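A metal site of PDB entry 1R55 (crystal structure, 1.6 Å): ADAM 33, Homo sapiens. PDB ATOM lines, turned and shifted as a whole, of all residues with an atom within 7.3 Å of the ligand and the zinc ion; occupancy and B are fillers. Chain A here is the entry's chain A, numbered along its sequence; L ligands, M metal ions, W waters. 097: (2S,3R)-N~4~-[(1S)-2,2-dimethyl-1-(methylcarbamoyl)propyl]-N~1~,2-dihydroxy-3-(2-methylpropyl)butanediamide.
N of Val 108 lies within hydrogen-bond range of O1 of the ligand (2.8 Å). O of Ala 106 lies within hydrogen-bond range of N2 of the ligand (3.0 Å). A nitrogen (N1) of the ligand lies close to the backbone carbonyl oxygen of Ala 172. A nitrogen (N3) of the ligand lies within hydrogen-bond range of the side-chain carboxylate (OE2) of Glu 143 (3.3 Å). A nitrogen (N3) of the ligand is in hydrogen-bond range of the backbone carbonyl oxygen of Gly 109. O2 of the ligand sits at hydrogen-bond distance from N of Thr 174, 2.9 Å away.
The backbone NH (N) of Leu 110 lies close to the side-chain carboxylate (OE2) of Glu 143 (3.5 Å). OG1 of Thr 139 sits at hydrogen-bond distance from NE2 of His 129, 3.0 Å away. The backbone carbonyl oxygen (O) of Leu 150 lies within hydrogen-bond range of a ring nitrogen (ND1) of His 146, at 3.1 Å. The backbone carbonyl oxygen of Ala 171 lies close to a ring nitrogen (ND1) of His 142 (3.4 Å). A ring nitrogen (ND1) of His 142 lies within hydrogen-bond range of the backbone carbonyl oxygen (O) of Val 169, at 2.9 Å. The side-chain hydroxyl (OG1) of Thr 139 lies within hydrogen-bond range of the backbone carbonyl oxygen (O) of Gly 135 (3.5 Å). The side-chain carboxylate (OE1) of Glu 143 is in hydrogen-bond range of the backbone NH (N) of Ala 111 (3.5 Å).
Merely in contact with the ligand: Ala 173 (3.4 Å), Thr 107 (3.4 Å), Ala 171 (3.5 Å) and Thr 139 (3.5 Å). Hydrophobic or aromatic side chains that line the ligand: Ala 106, Val 108, His 142, His 146, His 152 and Ala 173. 13 residues have an atom within 4 Å of the ligand: Ala 106, Thr 107, Val 108, Gly 109, Thr 139, His 142, Glu 143, His 146, His 152, Ala 171, Ala 172, Ala 173 and Thr 174. The nearest printed residue that does not touch the ligand is Leu 110 (4.1 Å).
Of the 28 residues printed, 3 come within 4 Å of the zinc ion.
The zinc ion is bound by O4 of the ligand (1.9 Å), NE2 of His 146 (2.0 Å), O3 of the ligand (2.1 Å), NE2 of His 152 (2.1 Å), NE2 of His 142 (2.2 Å) and water W2 (2.4 Å). The zinc ion has six donor atoms within binding distance.
Water W3 bridges O5 of the ligand (2.7 Å) and O of Ala 172 (2.9 Å). Water W1 bridges N3 of the ligand (3.3 Å) and N of Ala 111 (3.3 Å). Water W5 bridges the side-chain hydroxyl of Thr 107 (2.7 Å) and an oxygen (O5) of the ligand (2.8 Å).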
ATOM      1  N   GLY A 105     -12.090 -33.981  17.663  1.00  0.00           N
ATOM      2  CA  GLY A 105     -10.735 -34.404  17.973  1.00  0.00           C
ATOM      3  C   GLY A 105      -9.844 -33.367  18.632  1.00  0.00           C
ATOM      4  O   GLY A 105      -8.633 -33.543  18.718  1.00  0.00           O
ATOM      5  N   ALA A 106     -10.454 -32.279  19.098  1.00  0.00           N
ATOM      6  CA  ALA A 106      -9.724 -31.195  19.763  1.00  0.00           C
ATOM      7  C   ALA A 106      -8.732 -30.483  18.838  1.00  0.00           C
ATOM      8  O   ALA A 106      -7.904 -29.701  19.290  1.00  0.00           O
ATOM      9  CB  ALA A 106      -8.990 -31.737  20.991  1.00  0.00           C
ATOM     10  N   THR A 107      -8.821 -30.752  17.538  1.00  0.00           N
ATOM     11  CA  THR A 107      -7.942 -30.121  16.579  1.00  0.00           C
ATOM     12  C   THR A 107      -8.322 -28.647  16.452  1.00  0.00           C
ATOM     13  O   THR A 107      -9.502 -28.326  16.311  1.00  0.00           O
ATOM     14  CB  THR A 107      -8.054 -30.775  15.198  1.00  0.00           C
ATOM     15  OG1 THR A 107      -7.655 -32.154  15.284  1.00  0.00           O
ATOM     16  CG2 THR A 107      -7.166 -30.068  14.187  1.00  0.00           C
ATOM     17  N   VAL A 108      -7.329 -27.767  16.493  1.00  0.00           N
ATOM     18  CA  VAL A 108      -7.613 -26.334  16.373  1.00  0.00           C
ATOM     19  C   VAL A 108      -7.105 -25.725  15.066  1.00  0.00           C
ATOM     20  O   VAL A 108      -7.448 -24.584  14.749  1.00  0.00           O
ATOM     21  CB  VAL A 108      -7.041 -25.524  17.568  1.00  0.00           C
ATOM     22  CG1 VAL A 108      -7.823 -25.844  18.827  1.00  0.00           C
ATOM     23  CG2 VAL A 108      -5.562 -25.834  17.776  1.00  0.00           C
ATOM     24  N   GLY A 109      -6.311 -26.476  14.310  1.00  0.00           N
ATOM     25  CA  GLY A 109      -5.804 -25.973  13.053  1.00  0.00           C
ATOM     26  C   GLY A 109      -5.162 -27.039  12.178  1.00  0.00           C
ATOM     27  O   GLY A 109      -4.696 -28.061  12.688  1.00  0.00           O
ATOM     28  N   LEU A 110      -5.139 -26.798  10.866  1.00  0.00           N
ATOM     29  CA  LEU A 110      -4.563 -27.727   9.891  1.00  0.00           C
ATOM     30  C   LEU A 110      -4.049 -26.972   8.659  1.00  0.00           C
ATOM     31  O   LEU A 110      -4.542 -25.905   8.330  1.00  0.00           O
ATOM     32  CB  LEU A 110      -5.612 -28.724   9.399  1.00  0.00           C
ATOM     33  CG  LEU A 110      -5.877 -29.899  10.336  1.00  0.00           C
ATOM     34  CD1 LEU A 110      -6.977 -30.791   9.750  1.00  0.00           C
ATOM     35  CD2 LEU A 110      -4.616 -30.712  10.578  1.00  0.00           C
ATOM     36  N   ALA A 111      -3.084 -27.568   7.965  1.00  0.00           N
ATOM     37  CA  ALA A 111      -2.520 -26.975   6.751  1.00  0.00           C
ATOM     38  C   ALA A 111      -1.692 -28.018   6.007  1.00  0.00           C
ATOM     39  O   ALA A 111      -1.068 -28.878   6.610  1.00  0.00           O
ATOM     40  CB  ALA A 111      -1.639 -25.781   7.111  1.00  0.00           C
ATOM     41  N   VAL A 125      -6.413 -23.511   8.010  1.00  0.00           N
ATOM     42  CA  VAL A 125      -7.620 -23.197   8.772  1.00  0.00           C
ATOM     43  C   VAL A 125      -7.298 -23.212  10.261  1.00  0.00           C
ATOM     44  O   VAL A 125      -6.500 -24.040  10.712  1.00  0.00           O
ATOM     45  CB  VAL A 125      -8.765 -24.196   8.472  1.00  0.00           C
ATOM     46  CG1 VAL A 125      -8.350 -25.612   8.856  1.00  0.00           C
ATOM     47  CG2 VAL A 125     -10.021 -23.795   9.240  1.00  0.00           C
ATOM     48  N   SER A 126      -7.906 -22.310  11.011  1.00  0.00           N
ATOM     49  CA  SER A 126      -7.681 -22.202  12.448  1.00  0.00           C
ATOM     50  C   SER A 126      -8.976 -21.827  13.159  1.00  0.00           C
ATOM     51  O   SER A 126      -9.743 -21.011  12.665  1.00  0.00           O
ATOM     52  CB  SER A 126      -6.649 -21.100  12.746  1.00  0.00           C
ATOM     53  OG  SER A 126      -5.426 -21.307  12.078  1.00  0.00           O
ATOM     54  N   HIS A 129     -10.134 -20.216  19.073  1.00  0.00           N
ATOM     55  CA  HIS A 129     -10.369 -20.916  20.336  1.00  0.00           C
ATOM     56  C   HIS A 129     -10.133 -20.197  21.658  1.00  0.00           C
ATOM     57  O   HIS A 129     -10.596 -20.665  22.703  1.00  0.00           O
ATOM     58  CB  HIS A 129      -9.566 -22.210  20.314  1.00  0.00           C
ATOM     59  CG  HIS A 129      -8.094 -22.012  20.104  1.00  0.00           C
ATOM     60  ND1 HIS A 129      -7.230 -21.670  21.119  1.00  0.00           N
ATOM     61  CD2 HIS A 129      -7.341 -22.117  18.979  1.00  0.00           C
ATOM     62  CE1 HIS A 129      -6.004 -21.569  20.636  1.00  0.00           C
ATOM     63  NE2 HIS A 129      -6.043 -21.844  19.342  1.00  0.00           N
ATOM     64  N   GLY A 135      -3.992 -16.462  20.740  1.00  0.00           N
ATOM     65  CA  GLY A 135      -4.272 -17.889  20.669  1.00  0.00           C
ATOM     66  C   GLY A 135      -4.440 -18.320  19.222  1.00  0.00           C
ATOM     67  O   GLY A 135      -3.729 -19.198  18.729  1.00  0.00           O
ATOM     68  N   ALA A 136      -5.386 -17.689  18.544  1.00  0.00           N
ATOM     69  CA  ALA A 136      -5.654 -17.977  17.134  1.00  0.00           C
ATOM     70  C   ALA A 136      -4.422 -17.689  16.282  1.00  0.00           C
ATOM     71  O   ALA A 136      -4.130 -18.413  15.333  1.00  0.00           O
ATOM     72  CB  ALA A 136      -6.822 -17.142  16.649  1.00  0.00           C
ATOM     73  N   ALA A 138      -1.222 -17.859  17.150  1.00  0.00           N
ATOM     74  CA  ALA A 138      -0.203 -18.884  17.306  1.00  0.00           C
ATOM     75  C   ALA A 138      -0.580 -20.118  16.501  1.00  0.00           C
ATOM     76  O   ALA A 138       0.295 -20.798  15.958  1.00  0.00           O
ATOM     77  CB  ALA A 138      -0.040 -19.233  18.779  1.00  0.00           C
ATOM     78  N   THR A 139      -1.872 -20.414  16.421  1.00  0.00           N
ATOM     79  CA  THR A 139      -2.332 -21.556  15.653  1.00  0.00           C
ATOM     80  C   THR A 139      -2.114 -21.271  14.169  1.00  0.00           C
ATOM     81  O   THR A 139      -1.595 -22.095  13.431  1.00  0.00           O
ATOM     82  CB  THR A 139      -3.831 -21.836  15.923  1.00  0.00           C
ATOM     83  OG1 THR A 139      -3.992 -22.314  17.261  1.00  0.00           O
ATOM     84  CG2 THR A 139      -4.378 -22.880  14.950  1.00  0.00           C
ATOM     85  N   MET A 140      -2.501 -20.072  13.740  1.00  0.00           N
ATOM     86  CA  MET A 140      -2.346 -19.690  12.341  1.00  0.00           C
ATOM     87  C   MET A 140      -0.874 -19.686  11.932  1.00  0.00           C
ATOM     88  O   MET A 140      -0.528 -20.116  10.832  1.00  0.00           O
ATOM     89  CB  MET A 140      -2.964 -18.315  12.089  1.00  0.00           C
ATOM     90  CG  MET A 140      -3.105 -17.962  10.617  1.00  0.00           C
ATOM     91  SD  MET A 140      -3.996 -16.422  10.361  1.00  0.00           S
ATOM     92  CE  MET A 140      -5.645 -16.897  10.792  1.00  0.00           C
ATOM     93  N   HIS A 142       1.392 -21.490  13.216  1.00  0.00           N
ATOM     94  CA  HIS A 142       1.781 -22.897  13.229  1.00  0.00           C
ATOM     95  C   HIS A 142       1.418 -23.515  11.876  1.00  0.00           C
ATOM     96  O   HIS A 142       2.230 -24.240  11.282  1.00  0.00           O
ATOM     97  CB  HIS A 142       1.028 -23.635  14.347  1.00  0.00           C
ATOM     98  CG  HIS A 142       1.319 -25.105  14.428  1.00  0.00           C
ATOM     99  ND1 HIS A 142       2.215 -25.644  15.324  1.00  0.00           N
ATOM    100  CD2 HIS A 142       0.809 -26.142  13.730  1.00  0.00           C
ATOM    101  CE1 HIS A 142       2.234 -26.955  15.188  1.00  0.00           C
ATOM    102  NE2 HIS A 142       1.390 -27.291  14.223  1.00  0.00           N
ATOM    103  N   GLU A 143       0.220 -23.224  11.383  1.00  0.00           N
ATOM    104  CA  GLU A 143      -0.197 -23.766  10.093  1.00  0.00           C
ATOM    105  C   GLU A 143       0.627 -23.171   8.953  1.00  0.00           C
ATOM    106  O   GLU A 143       0.951 -23.857   7.975  1.00  0.00           O
ATOM    107  CB  GLU A 143      -1.692 -23.522   9.850  1.00  0.00           C
ATOM    108  CG  GLU A 143      -2.627 -23.992  10.958  1.00  0.00           C
ATOM    109  CD  GLU A 143      -2.249 -25.339  11.570  1.00  0.00           C
ATOM    110  OE1 GLU A 143      -1.698 -26.206  10.873  1.00  0.00           O
ATOM    111  OE2 GLU A 143      -2.529 -25.526  12.777  1.00  0.00           O
ATOM    112  N   HIS A 146       3.830 -25.092   8.740  1.00  0.00           N
ATOM    113  CA  HIS A 146       3.750 -26.330   7.987  1.00  0.00           C
ATOM    114  C   HIS A 146       3.820 -26.023   6.494  1.00  0.00           C
ATOM    115  O   HIS A 146       4.457 -26.745   5.737  1.00  0.00           O
ATOM    116  CB  HIS A 146       2.445 -27.082   8.268  1.00  0.00           C
ATOM    117  CG  HIS A 146       2.439 -27.836   9.569  1.00  0.00           C
ATOM    118  ND1 HIS A 146       3.417 -28.750   9.898  1.00  0.00           N
ATOM    119  CD2 HIS A 146       1.572 -27.821  10.600  1.00  0.00           C
ATOM    120  CE1 HIS A 146       3.137 -29.276  11.084  1.00  0.00           C
ATOM    121  NE2 HIS A 146       2.022 -28.727  11.529  1.00  0.00           N
ATOM    122  N   LEU A 150       7.917 -26.602   7.780  1.00  0.00           N
ATOM    123  CA  LEU A 150       8.376 -26.777   9.148  1.00  0.00           C
ATOM    124  C   LEU A 150       7.649 -27.936   9.796  1.00  0.00           C
ATOM    125  O   LEU A 150       6.446 -28.105   9.625  1.00  0.00           O
ATOM    126  CB  LEU A 150       8.122 -25.500   9.974  1.00  0.00           C
ATOM    127  CG  LEU A 150       8.699 -24.243   9.318  1.00  0.00           C
ATOM    128  CD1 LEU A 150       8.552 -23.045  10.251  1.00  0.00           C
ATOM    129  CD2 LEU A 150      10.170 -24.427   8.947  1.00  0.00           C
ATOM    130  N   SER A 151       8.380 -28.758  10.542  1.00  0.00           N
ATOM    131  CA  SER A 151       7.780 -29.894  11.212  1.00  0.00           C
ATOM    132  C   SER A 151       7.541 -29.522  12.672  1.00  0.00           C
ATOM    133  O   SER A 151       7.937 -28.447  13.113  1.00  0.00           O
ATOM    134  CB  SER A 151       8.709 -31.108  11.147  1.00  0.00           C
ATOM    135  OG  SER A 151       9.826 -30.907  11.984  1.00  0.00           O
ATOM    136  N   HIS A 152       6.874 -30.402  13.407  1.00  0.00           N
ATOM    137  CA  HIS A 152       6.648 -30.138  14.816  1.00  0.00           C
ATOM    138  C   HIS A 152       8.015 -30.214  15.494  1.00  0.00           C
ATOM    139  O   HIS A 152       8.875 -31.014  15.087  1.00  0.00           O
ATOM    140  CB  HIS A 152       5.697 -31.171  15.410  1.00  0.00           C
ATOM    141  CG  HIS A 152       4.268 -30.969  15.026  1.00  0.00           C
ATOM    142  ND1 HIS A 152       3.265 -31.877  15.334  1.00  0.00           N
ATOM    143  CD2 HIS A 152       3.656 -29.961  14.355  1.00  0.00           C
ATOM    144  CE1 HIS A 152       2.115 -31.432  14.885  1.00  0.00           C
ATOM    145  NE2 HIS A 152       2.315 -30.268  14.286  1.00  0.00           N
ATOM    146  N   VAL A 169       6.321 -21.886  18.571  1.00  0.00           N
ATOM    147  CA  VAL A 169       5.188 -22.055  17.671  1.00  0.00           C
ATOM    148  C   VAL A 169       4.965 -23.452  17.098  1.00  0.00           C
ATOM    149  O   VAL A 169       3.826 -23.890  16.976  1.00  0.00           O
ATOM    150  CB  VAL A 169       5.267 -21.028  16.507  1.00  0.00           C
ATOM    151  CG1 VAL A 169       4.116 -21.236  15.534  1.00  0.00           C
ATOM    152  CG2 VAL A 169       5.230 -19.615  17.071  1.00  0.00           C
ATOM    153  N   MET A 170       6.032 -24.160  16.737  1.00  0.00           N
ATOM    154  CA  MET A 170       5.835 -25.490  16.171  1.00  0.00           C
ATOM    155  C   MET A 170       5.628 -26.642  17.154  1.00  0.00           C
ATOM    156  O   MET A 170       5.851 -27.807  16.813  1.00  0.00           O
ATOM    157  CB  MET A 170       6.964 -25.828  15.185  1.00  0.00           C
ATOM    158  CG  MET A 170       6.969 -24.948  13.923  1.00  0.00           C
ATOM    159  SD  MET A 170       5.341 -24.642  13.160  1.00  0.00           S
ATOM    160  CE  MET A 170       4.850 -26.296  12.665  1.00  0.00           C
ATOM    161  N   ALA A 171       5.198 -26.325  18.371  1.00  0.00           N
ATOM    162  CA  ALA A 171       4.917 -27.375  19.342  1.00  0.00           C
ATOM    163  C   ALA A 171       3.687 -28.098  18.795  1.00  0.00           C
ATOM    164  O   ALA A 171       2.877 -27.491  18.097  1.00  0.00           O
ATOM    165  CB  ALA A 171       4.625 -26.767  20.702  1.00  0.00           C
ATOM    166  N   ALA A 172       3.538 -29.380  19.133  1.00  0.00           N
ATOM    167  CA  ALA A 172       2.415 -30.174  18.648  1.00  0.00           C
ATOM    168  C   ALA A 172       1.088 -29.888  19.348  1.00  0.00           C
ATOM    169  O   ALA A 172       0.020 -30.204  18.826  1.00  0.00           O
ATOM    170  CB  ALA A 172       2.746 -31.660  18.785  1.00  0.00           C
ATOM    171  N   ALA A 173       1.170 -29.278  20.521  1.00  0.00           N
ATOM    172  CA  ALA A 173      -0.004 -28.942  21.296  1.00  0.00           C
ATOM    173  C   ALA A 173       0.039 -27.466  21.648  1.00  0.00           C
ATOM    174  O   ALA A 173       1.117 -26.883  21.765  1.00  0.00           O
ATOM    175  CB  ALA A 173      -0.052 -29.779  22.571  1.00  0.00           C
ATOM    176  N   THR A 174      -1.135 -26.861  21.812  1.00  0.00           N
ATOM    177  CA  THR A 174      -1.168 -25.447  22.151  1.00  0.00           C
ATOM    178  C   THR A 174      -2.038 -25.179  23.365  1.00  0.00           C
ATOM    179  O   THR A 174      -2.824 -26.025  23.799  1.00  0.00           O
ATOM    180  CB  THR A 174      -1.668 -24.600  20.961  1.00  0.00           C
ATOM    181  OG1 THR A 174      -1.375 -23.219  21.210  1.00  0.00           O
ATOM    182  CG2 THR A 174      -3.166 -24.757  20.775  1.00  0.00           C
ATOM    183  N   GLY A 175      -1.890 -23.977  23.907  1.00  0.00           N
ATOM    184  CA  GLY A 175      -2.649 -23.586  25.075  1.00  0.00           C
ATOM    185  C   GLY A 175      -1.930 -22.429  25.744  1.00  0.00           C
ATOM    186  O   GLY A 175      -0.745 -22.207  25.495  1.00  0.00           O
HETATM  187  N1  097 L   1      -3.297 -29.653  18.581  1.00  0.00           N
HETATM  188  C2  097 L   1      -0.609 -27.026  17.974  1.00  0.00           C
HETATM  189  O2  097 L   1      -3.383 -28.647  21.265  1.00  0.00           O
HETATM  190  C4  097 L   1      -3.657 -29.113  17.400  1.00  0.00           C
HETATM  191  O3  097 L   1      -0.851 -28.431  12.319  1.00  0.00           O
HETATM  192  C5  097 L   1      -4.371 -29.961  19.519  1.00  0.00           C
HETATM  193  C6  097 L   1      -4.207 -31.395  20.043  1.00  0.00           C
HETATM  194  C8  097 L   1      -2.812 -31.556  20.669  1.00  0.00           C
HETATM  195  C9  097 L   1      -5.295 -31.701  21.082  1.00  0.00           C
HETATM  196  C10 097 L   1      -4.416 -28.969  20.663  1.00  0.00           C
HETATM  197  C11 097 L   1      -5.804 -27.575  22.060  1.00  0.00           C
HETATM  198  N3  097 L   1      -1.968 -28.733  13.058  1.00  0.00           N
HETATM  199  C12 097 L   1      -1.628 -29.420  14.160  1.00  0.00           C
HETATM  200  O4  097 L   1      -0.488 -29.823  14.356  1.00  0.00           O
HETATM  201  C13 097 L   1      -2.717 -29.651  15.175  1.00  0.00           C
HETATM  202  O5  097 L   1      -2.880 -31.034  15.431  1.00  0.00           O
HETATM  203  C14 097 L   1      -2.484 -28.865  16.461  1.00  0.00           C
HETATM  204  C15 097 L   1      -2.350 -27.366  16.173  1.00  0.00           C
HETATM  205  C1  097 L   1      -1.920 -26.519  17.384  1.00  0.00           C
HETATM  206  C3  097 L   1      -1.766 -25.059  16.981  1.00  0.00           C
HETATM  207  O1  097 L   1      -4.802 -28.834  17.074  1.00  0.00           O
HETATM  208  C7  097 L   1      -4.349 -32.366  18.852  1.00  0.00           C
HETATM  209  N2  097 L   1      -5.645 -28.487  20.925  1.00  0.00           N
HETATM  210 ZN    ZN M   1       0.910 -29.129  13.198  1.00  0.00          ZN
HETATM  211  O   HOH W   1      -1.518 -29.638   9.953  1.00  0.00           O
HETATM  212  O   HOH W   2       0.437 -31.146  12.079  1.00  0.00           O
HETATM  213  O   HOH W   3      -0.810 -32.114  16.863  1.00  0.00           O
HETATM  214  O   HOH W   4      -3.496 -29.490  24.403  1.00  0.00           O
HETATM  215  O   HOH W   5      -5.002 -32.754  14.907  1.00  0.00           O
